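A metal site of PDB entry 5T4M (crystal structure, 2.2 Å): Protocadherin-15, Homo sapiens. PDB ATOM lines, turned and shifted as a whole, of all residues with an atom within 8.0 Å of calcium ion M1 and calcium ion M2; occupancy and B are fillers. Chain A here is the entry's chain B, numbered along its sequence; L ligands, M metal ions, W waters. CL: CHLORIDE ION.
N of Glu 129 sits at hydrogen-bond distance from OE1 of Glu 29 (2.7 Å).
The side-chain amide oxygen of Asn 131 lies close to the side-chain amide oxygen of Gln 132 (3.3 Å).
The side-chain carboxylate (OD1) of Asp 226 lies within hydrogen-bond range of the backbone NH (N) of Gln 229, 2.6 Å away.
The side-chain amide oxygen of Asn 130 sits close to the side-chain amide oxygen of Gln 229, at 3.4 Å.
OD1 of Asp 226 is in hydrogen-bond range of N of Val 228 (2.9 Å).
Water W2 bridges the side-chain carboxylate of Glu 29 (2.7 Å) and the side-chain amide nitrogen of Asn 131 (2.9 Å).
Calcium ion M1 is bound by the side-chain amide oxygen (OD1) of Asn 131, the side-chain carboxylate (OD1) of Asp 173, the backbone carbonyl oxygen (O) of Glu 129, the side-chain carboxylate (OD1) of Asp 128, water W2, the side-chain carboxylate (OD2) of Asp 128 and a chlorine (CL) of the ligand.
Calcium ion M1 has seven donor atoms within binding distance.
Calcium ion M2 is bound by the side-chain amide oxygen (OD1) of Asn 130 (2.3 Å), the backbone carbonyl oxygen (O) of Gln 132 (2.3 Å), the side-chain carboxylate (OD1) of Asp 171 (2.3 Å), the side-chain carboxylate (OD2) of Asp 226 (2.4 Å), the side-chain carboxylate (OD2) of Asp 173 (2.4 Å), water W1 (2.4 Å) and the side-chain carboxylate (OD2) of Asp 171 (2.4 Å).
The nearest printed residue that does not touch calcium ion M1 is Glu 29 (4.1 Å).
The nearest printed residue that does not touch calcium ion M2 is Gln 229 (4.3 Å).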
ATOM      1  N   GLU A  29       3.118  10.746  -5.634  1.00  0.00           N
ATOM      2  CA  GLU A  29       3.953  10.663  -6.824  1.00  0.00           C
ATOM      3  C   GLU A  29       3.112  10.734  -8.088  1.00  0.00           C
ATOM      4  O   GLU A  29       1.919  10.415  -8.067  1.00  0.00           O
ATOM      5  CB  GLU A  29       4.723   9.342  -6.857  1.00  0.00           C
ATOM      6  CG  GLU A  29       3.822   8.126  -6.987  1.00  0.00           C
ATOM      7  CD  GLU A  29       4.578   6.871  -7.381  1.00  0.00           C
ATOM      8  OE1 GLU A  29       4.105   5.763  -7.021  1.00  0.00           O
ATOM      9  OE2 GLU A  29       5.621   6.980  -8.052  1.00  0.00           O
ATOM     10  N   LEU A  30       3.734  11.141  -9.183  1.00  0.00           N
ATOM     11  CA  LEU A  30       3.124  11.085 -10.522  1.00  0.00           C
ATOM     12  C   LEU A  30       1.895  11.989 -10.618  1.00  0.00           C
ATOM     13  O   LEU A  30       0.977  11.709 -11.388  1.00  0.00           O
ATOM     14  CB  LEU A  30       2.745   9.651 -10.886  1.00  0.00           C
ATOM     15  CG  LEU A  30       3.885   8.630 -10.837  1.00  0.00           C
ATOM     16  CD1 LEU A  30       3.373   7.237 -11.159  1.00  0.00           C
ATOM     17  CD2 LEU A  30       4.999   9.038 -11.788  1.00  0.00           C
ATOM     18  N   ARG A  96       8.444   8.193  -7.725  1.00  0.00           N
ATOM     19  CA  ARG A  96       8.918   7.656  -6.463  1.00  0.00           C
ATOM     20  C   ARG A  96      10.016   6.602  -6.660  1.00  0.00           C
ATOM     21  O   ARG A  96      10.739   6.282  -5.711  1.00  0.00           O
ATOM     22  CB  ARG A  96       7.759   7.066  -5.655  1.00  0.00           C
ATOM     23  CG  ARG A  96       8.086   6.928  -4.184  1.00  0.00           C
ATOM     24  CD  ARG A  96       6.902   6.463  -3.371  1.00  0.00           C
ATOM     25  NE  ARG A  96       7.282   6.224  -1.983  1.00  0.00           N
ATOM     26  CZ  ARG A  96       7.821   5.100  -1.549  1.00  0.00           C
ATOM     27  NH1 ARG A  96       8.044   4.094  -2.387  1.00  0.00           N
ATOM     28  NH2 ARG A  96       8.140   4.965  -0.272  1.00  0.00           N
ATOM     29  N   ASP A  97      10.138   6.087  -7.874  1.00  0.00           N
ATOM     30  CA  ASP A  97      11.210   5.147  -8.204  1.00  0.00           C
ATOM     31  C   ASP A  97      12.591   5.777  -8.032  1.00  0.00           C
ATOM     32  O   ASP A  97      13.584   5.083  -7.798  1.00  0.00           O
ATOM     33  CB  ASP A  97      11.063   4.649  -9.641  1.00  0.00           C
ATOM     34  CG  ASP A  97      10.143   3.447  -9.748  1.00  0.00           C
ATOM     35  OD1 ASP A  97       9.364   3.197  -8.804  1.00  0.00           O
ATOM     36  OD2 ASP A  97      10.187   2.756 -10.792  1.00  0.00           O
ATOM     37  N   LEU A 127       4.698   9.917  -1.624  1.00  0.00           N
ATOM     38  CA  LEU A 127       3.790   8.804  -1.386  1.00  0.00           C
ATOM     39  C   LEU A 127       3.603   7.934  -2.622  1.00  0.00           C
ATOM     40  O   LEU A 127       3.456   8.433  -3.731  1.00  0.00           O
ATOM     41  CB  LEU A 127       2.432   9.319  -0.908  1.00  0.00           C
ATOM     42  CG  LEU A 127       2.459  10.151   0.375  1.00  0.00           C
ATOM     43  CD1 LEU A 127       1.094  10.769   0.638  1.00  0.00           C
ATOM     44  CD2 LEU A 127       2.907   9.297   1.558  1.00  0.00           C
ATOM     45  N   ASP A 128       3.607   6.611  -2.426  1.00  0.00           N
ATOM     46  CA  ASP A 128       3.435   5.679  -3.531  1.00  0.00           C
ATOM     47  C   ASP A 128       2.044   5.776  -4.133  1.00  0.00           C
ATOM     48  O   ASP A 128       1.085   6.103  -3.449  1.00  0.00           O
ATOM     49  CB  ASP A 128       3.699   4.240  -3.083  1.00  0.00           C
ATOM     50  CG  ASP A 128       3.606   3.246  -4.229  1.00  0.00           C
ATOM     51  OD1 ASP A 128       4.312   3.440  -5.239  1.00  0.00           O
ATOM     52  OD2 ASP A 128       2.825   2.283  -4.134  1.00  0.00           O
ATOM     53  N   GLU A 129       1.957   5.484  -5.424  1.00  0.00           N
ATOM     54  CA  GLU A 129       0.677   5.368  -6.093  1.00  0.00           C
ATOM     55  C   GLU A 129       0.259   3.897  -6.146  1.00  0.00           C
ATOM     56  O   GLU A 129       1.042   3.041  -6.573  1.00  0.00           O
ATOM     57  CB  GLU A 129       0.738   5.962  -7.505  1.00  0.00           C
ATOM     58  CG  GLU A 129      -0.608   6.098  -8.179  1.00  0.00           C
ATOM     59  CD  GLU A 129      -0.489   6.556  -9.620  1.00  0.00           C
ATOM     60  OE1 GLU A 129      -1.023   7.638  -9.952  1.00  0.00           O
ATOM     61  OE2 GLU A 129       0.145   5.832 -10.419  1.00  0.00           O
ATOM     62  N   ASN A 130      -0.964   3.614  -5.716  1.00  0.00           N
ATOM     63  CA  ASN A 130      -1.522   2.262  -5.774  1.00  0.00           C
ATOM     64  C   ASN A 130      -1.762   1.866  -7.235  1.00  0.00           C
ATOM     65  O   ASN A 130      -2.849   2.086  -7.769  1.00  0.00           O
ATOM     66  CB  ASN A 130      -2.820   2.176  -4.972  1.00  0.00           C
ATOM     67  CG  ASN A 130      -3.371   0.758  -4.876  1.00  0.00           C
ATOM     68  OD1 ASN A 130      -2.925  -0.161  -5.570  1.00  0.00           O
ATOM     69  ND2 ASN A 130      -4.349   0.576  -4.001  1.00  0.00           N
ATOM     70  N   ASN A 131      -0.746   1.291  -7.863  1.00  0.00           N
ATOM     71  CA  ASN A 131      -0.831   0.978  -9.289  1.00  0.00           C
ATOM     72  C   ASN A 131      -0.500  -0.469  -9.624  1.00  0.00           C
ATOM     73  O   ASN A 131      -0.389  -0.832 -10.787  1.00  0.00           O
ATOM     74  CB  ASN A 131       0.089   1.920 -10.083  1.00  0.00           C
ATOM     75  CG  ASN A 131       1.431   2.123  -9.412  1.00  0.00           C
ATOM     76  OD1 ASN A 131       1.844   1.357  -8.540  1.00  0.00           O
ATOM     77  ND2 ASN A 131       2.132   3.184  -9.825  1.00  0.00           N
ATOM     78  N   GLN A 132      -0.347  -1.298  -8.589  1.00  0.00           N
ATOM     79  CA  GLN A 132      -0.146  -2.731  -8.800  1.00  0.00           C
ATOM     80  C   GLN A 132      -1.382  -3.514  -8.358  1.00  0.00           C
ATOM     81  O   GLN A 132      -1.873  -3.328  -7.254  1.00  0.00           O
ATOM     82  CB  GLN A 132       1.077  -3.237  -8.036  1.00  0.00           C
ATOM     83  CG  GLN A 132       2.363  -2.476  -8.341  1.00  0.00           C
ATOM     84  CD  GLN A 132       2.620  -2.335  -9.823  1.00  0.00           C
ATOM     85  OE1 GLN A 132       2.802  -1.225 -10.338  1.00  0.00           O
ATOM     86  NE2 GLN A 132       2.646  -3.456 -10.528  1.00  0.00           N
ATOM     87  N   SER A 133      -1.887  -4.378  -9.242  1.00  0.00           N
ATOM     88  CA  SER A 133      -3.009  -5.236  -8.907  1.00  0.00           C
ATOM     89  C   SER A 133      -2.609  -6.254  -7.844  1.00  0.00           C
ATOM     90  O   SER A 133      -1.486  -6.760  -7.874  1.00  0.00           O
ATOM     91  CB  SER A 133      -3.526  -5.976 -10.139  1.00  0.00           C
ATOM     92  OG  SER A 133      -4.065  -5.078 -11.092  1.00  0.00           O
ATOM     93  N   PRO A 134      -3.511  -6.539  -6.901  1.00  0.00           N
ATOM     94  CA  PRO A 134      -3.236  -7.600  -5.934  1.00  0.00           C
ATOM     95  C   PRO A 134      -3.285  -8.956  -6.629  1.00  0.00           C
ATOM     96  O   PRO A 134      -3.783  -9.038  -7.741  1.00  0.00           O
ATOM     97  CB  PRO A 134      -4.367  -7.447  -4.912  1.00  0.00           C
ATOM     98  CG  PRO A 134      -5.476  -6.798  -5.663  1.00  0.00           C
ATOM     99  CD  PRO A 134      -4.821  -5.899  -6.669  1.00  0.00           C
ATOM    100  N   TYR A 135      -2.743  -9.992  -5.983  1.00  0.00           N
ATOM    101  CA  TYR A 135      -2.652 -11.310  -6.609  1.00  0.00           C
ATOM    102  C   TYR A 135      -2.564 -12.390  -5.551  1.00  0.00           C
ATOM    103  O   TYR A 135      -2.147 -12.128  -4.425  1.00  0.00           O
ATOM    104  CB  TYR A 135      -1.432 -11.384  -7.534  1.00  0.00           C
ATOM    105  CG  TYR A 135      -0.107 -11.286  -6.811  1.00  0.00           C
ATOM    106  CD1 TYR A 135       0.420 -10.046  -6.443  1.00  0.00           C
ATOM    107  CD2 TYR A 135       0.614 -12.430  -6.487  1.00  0.00           C
ATOM    108  CE1 TYR A 135       1.628  -9.967  -5.778  1.00  0.00           C
ATOM    109  CE2 TYR A 135       1.823 -12.351  -5.822  1.00  0.00           C
ATOM    110  CZ  TYR A 135       2.321 -11.111  -5.471  1.00  0.00           C
ATOM    111  OH  TYR A 135       3.529 -11.032  -4.806  1.00  0.00           O
ATOM    112  N   LEU A 170      -1.330 -11.007  -1.920  1.00  0.00           N
ATOM    113  CA  LEU A 170      -0.294  -9.980  -1.832  1.00  0.00           C
ATOM    114  C   LEU A 170      -0.539  -8.823  -2.787  1.00  0.00           C
ATOM    115  O   LEU A 170      -1.392  -8.902  -3.669  1.00  0.00           O
ATOM    116  CB  LEU A 170       1.078 -10.598  -2.101  1.00  0.00           C
ATOM    117  CG  LEU A 170       1.590 -11.567  -1.019  1.00  0.00           C
ATOM    118  CD1 LEU A 170       2.888 -12.217  -1.449  1.00  0.00           C
ATOM    119  CD2 LEU A 170       1.759 -10.840   0.316  1.00  0.00           C
ATOM    120  N   ASP A 171       0.240  -7.757  -2.617  1.00  0.00           N
ATOM    121  CA  ASP A 171       0.137  -6.569  -3.457  1.00  0.00           C
ATOM    122  C   ASP A 171       1.483  -5.846  -3.441  1.00  0.00           C
ATOM    123  O   ASP A 171       1.975  -5.445  -2.393  1.00  0.00           O
ATOM    124  CB  ASP A 171      -0.988  -5.650  -2.956  1.00  0.00           C
ATOM    125  CG  ASP A 171      -1.367  -4.569  -3.969  1.00  0.00           C
ATOM    126  OD1 ASP A 171      -0.472  -3.843  -4.449  1.00  0.00           O
ATOM    127  OD2 ASP A 171      -2.566  -4.473  -4.284  1.00  0.00           O
ATOM    128  N   LYS A 172       2.062  -5.668  -4.629  1.00  0.00           N
ATOM    129  CA  LYS A 172       3.417  -5.137  -4.756  1.00  0.00           C
ATOM    130  C   LYS A 172       3.550  -3.688  -4.294  1.00  0.00           C
ATOM    131  O   LYS A 172       4.658  -3.226  -4.011  1.00  0.00           O
ATOM    132  CB  LYS A 172       3.900  -5.259  -6.197  1.00  0.00           C
ATOM    133  CG  LYS A 172       4.250  -6.677  -6.621  1.00  0.00           C
ATOM    134  CD  LYS A 172       5.490  -7.187  -5.884  1.00  0.00           C
ATOM    135  CE  LYS A 172       5.787  -8.643  -6.227  1.00  0.00           C
ATOM    136  NZ  LYS A 172       6.033  -8.836  -7.678  1.00  0.00           N
ATOM    137  N   ASP A 173       2.433  -2.974  -4.214  1.00  0.00           N
ATOM    138  CA  ASP A 173       2.447  -1.584  -3.732  1.00  0.00           C
ATOM    139  C   ASP A 173       2.784  -1.525  -2.251  1.00  0.00           C
ATOM    140  O   ASP A 173       3.235  -0.505  -1.751  1.00  0.00           O
ATOM    141  CB  ASP A 173       1.096  -0.901  -3.983  1.00  0.00           C
ATOM    142  CG  ASP A 173       0.854  -0.616  -5.444  1.00  0.00           C
ATOM    143  OD1 ASP A 173       1.803  -0.188  -6.129  1.00  0.00           O
ATOM    144  OD2 ASP A 173      -0.289  -0.803  -5.916  1.00  0.00           O
ATOM    145  N   ILE A 174       2.556  -2.647  -1.574  1.00  0.00           N
ATOM    146  CA  ILE A 174       2.743  -2.736  -0.131  1.00  0.00           C
ATOM    147  C   ILE A 174       4.032  -3.479   0.206  1.00  0.00           C
ATOM    148  O   ILE A 174       4.308  -4.547  -0.349  1.00  0.00           O
ATOM    149  CB  ILE A 174       1.556  -3.446   0.547  1.00  0.00           C
ATOM    150  CG1 ILE A 174       0.239  -2.789   0.122  1.00  0.00           C
ATOM    151  CG2 ILE A 174       1.712  -3.457   2.053  1.00  0.00           C
ATOM    152  CD1 ILE A 174       0.204  -1.292   0.367  1.00  0.00           C
ATOM    153  N   PRO A 180      -1.444  -6.058   3.352  1.00  0.00           N
ATOM    154  CA  PRO A 180      -1.903  -5.202   2.249  1.00  0.00           C
ATOM    155  C   PRO A 180      -3.344  -4.730   2.436  1.00  0.00           C
ATOM    156  O   PRO A 180      -3.812  -3.890   1.663  1.00  0.00           O
ATOM    157  CB  PRO A 180      -1.779  -6.114   1.026  1.00  0.00           C
ATOM    158  CG  PRO A 180      -1.965  -7.492   1.575  1.00  0.00           C
ATOM    159  CD  PRO A 180      -1.327  -7.472   2.949  1.00  0.00           C
ATOM    160  N   LEU A 182      -6.302  -6.055   1.899  1.00  0.00           N
ATOM    161  CA  LEU A 182      -7.123  -6.240   0.726  1.00  0.00           C
ATOM    162  C   LEU A 182      -8.542  -6.645   1.091  1.00  0.00           C
ATOM    163  O   LEU A 182      -8.785  -7.173   2.177  1.00  0.00           O
ATOM    164  CB  LEU A 182      -6.496  -7.299  -0.190  1.00  0.00           C
ATOM    165  CG  LEU A 182      -5.052  -7.013  -0.577  1.00  0.00           C
ATOM    166  CD1 LEU A 182      -4.417  -8.227  -1.239  1.00  0.00           C
ATOM    167  CD2 LEU A 182      -5.002  -5.786  -1.487  1.00  0.00           C
ATOM    168  N   PHE A 225      -9.267  -7.039  -3.986  1.00  0.00           N
ATOM    169  CA  PHE A 225      -9.459  -5.643  -4.377  1.00  0.00           C
ATOM    170  C   PHE A 225      -8.657  -4.717  -3.475  1.00  0.00           C
ATOM    171  O   PHE A 225      -8.768  -4.790  -2.243  1.00  0.00           O
ATOM    172  CB  PHE A 225     -10.954  -5.301  -4.335  1.00  0.00           C
ATOM    173  CG  PHE A 225     -11.284  -3.897  -4.750  1.00  0.00           C
ATOM    174  CD1 PHE A 225     -10.998  -3.441  -6.025  1.00  0.00           C
ATOM    175  CD2 PHE A 225     -11.914  -3.029  -3.867  1.00  0.00           C
ATOM    176  CE1 PHE A 225     -11.314  -2.143  -6.415  1.00  0.00           C
ATOM    177  CE2 PHE A 225     -12.230  -1.736  -4.240  1.00  0.00           C
ATOM    178  CZ  PHE A 225     -11.934  -1.290  -5.519  1.00  0.00           C
ATOM    179  N   ASP A 226      -7.855  -3.839  -4.062  1.00  0.00           N
ATOM    180  CA  ASP A 226      -6.969  -2.984  -3.271  1.00  0.00           C
ATOM    181  C   ASP A 226      -7.483  -1.552  -3.179  1.00  0.00           C
ATOM    182  O   ASP A 226      -6.738  -0.630  -2.837  1.00  0.00           O
ATOM    183  CB  ASP A 226      -5.545  -2.987  -3.856  1.00  0.00           C
ATOM    184  CG  ASP A 226      -5.457  -2.323  -5.227  1.00  0.00           C
ATOM    185  OD1 ASP A 226      -6.498  -1.961  -5.813  1.00  0.00           O
ATOM    186  OD2 ASP A 226      -4.321  -2.165  -5.732  1.00  0.00           O
ATOM    187  N   GLY A 227      -8.760  -1.362  -3.485  1.00  0.00           N
ATOM    188  CA  GLY A 227      -9.350  -0.035  -3.474  1.00  0.00           C
ATOM    189  C   GLY A 227      -9.360   0.620  -4.851  1.00  0.00           C
ATOM    190  O   GLY A 227     -10.115   1.561  -5.090  1.00  0.00           O
ATOM    191  N   VAL A 228      -8.515   0.110  -5.744  1.00  0.00           N
ATOM    192  CA  VAL A 228      -8.399   0.671  -7.089  1.00  0.00           C
ATOM    193  C   VAL A 228      -8.511  -0.413  -8.173  1.00  0.00           C
ATOM    194  O   VAL A 228      -9.292  -0.272  -9.112  1.00  0.00           O
ATOM    195  CB  VAL A 228      -7.065   1.425  -7.276  1.00  0.00           C
ATOM    196  CG1 VAL A 228      -6.898   1.894  -8.707  1.00  0.00           C
ATOM    197  CG2 VAL A 228      -6.990   2.611  -6.321  1.00  0.00           C
ATOM    198  N   GLN A 229      -7.740  -1.487  -8.027  1.00  0.00           N
ATOM    199  CA  GLN A 229      -7.733  -2.572  -9.018  1.00  0.00           C
ATOM    200  C   GLN A 229      -8.118  -3.912  -8.396  1.00  0.00           C
ATOM    201  O   GLN A 229      -7.871  -4.169  -7.223  1.00  0.00           O
ATOM    202  CB  GLN A 229      -6.349  -2.689  -9.670  1.00  0.00           C
ATOM    203  CG  GLN A 229      -5.886  -1.431 -10.394  1.00  0.00           C
ATOM    204  CD  GLN A 229      -4.669  -0.792  -9.752  1.00  0.00           C
ATOM    205  OE1 GLN A 229      -4.411  -0.966  -8.558  1.00  0.00           O
ATOM    206  NE2 GLN A 229      -3.910  -0.052 -10.546  1.00  0.00           N
HETATM  207 CL    CL L   1       5.110   0.227  -6.061  1.00  0.00          CL
HETATM  208 CA    CA M   1       3.098   1.781  -6.558  1.00  0.00          CA
HETATM  209 CA    CA M   2      -2.017  -2.264  -5.190  1.00  0.00          CA
HETATM  210  O   HOH W   1      -2.143  -1.622  -2.852  1.00  0.00           O
HETATM  211  O   HOH W   2       4.341   3.320  -8.028  1.00  0.00           O
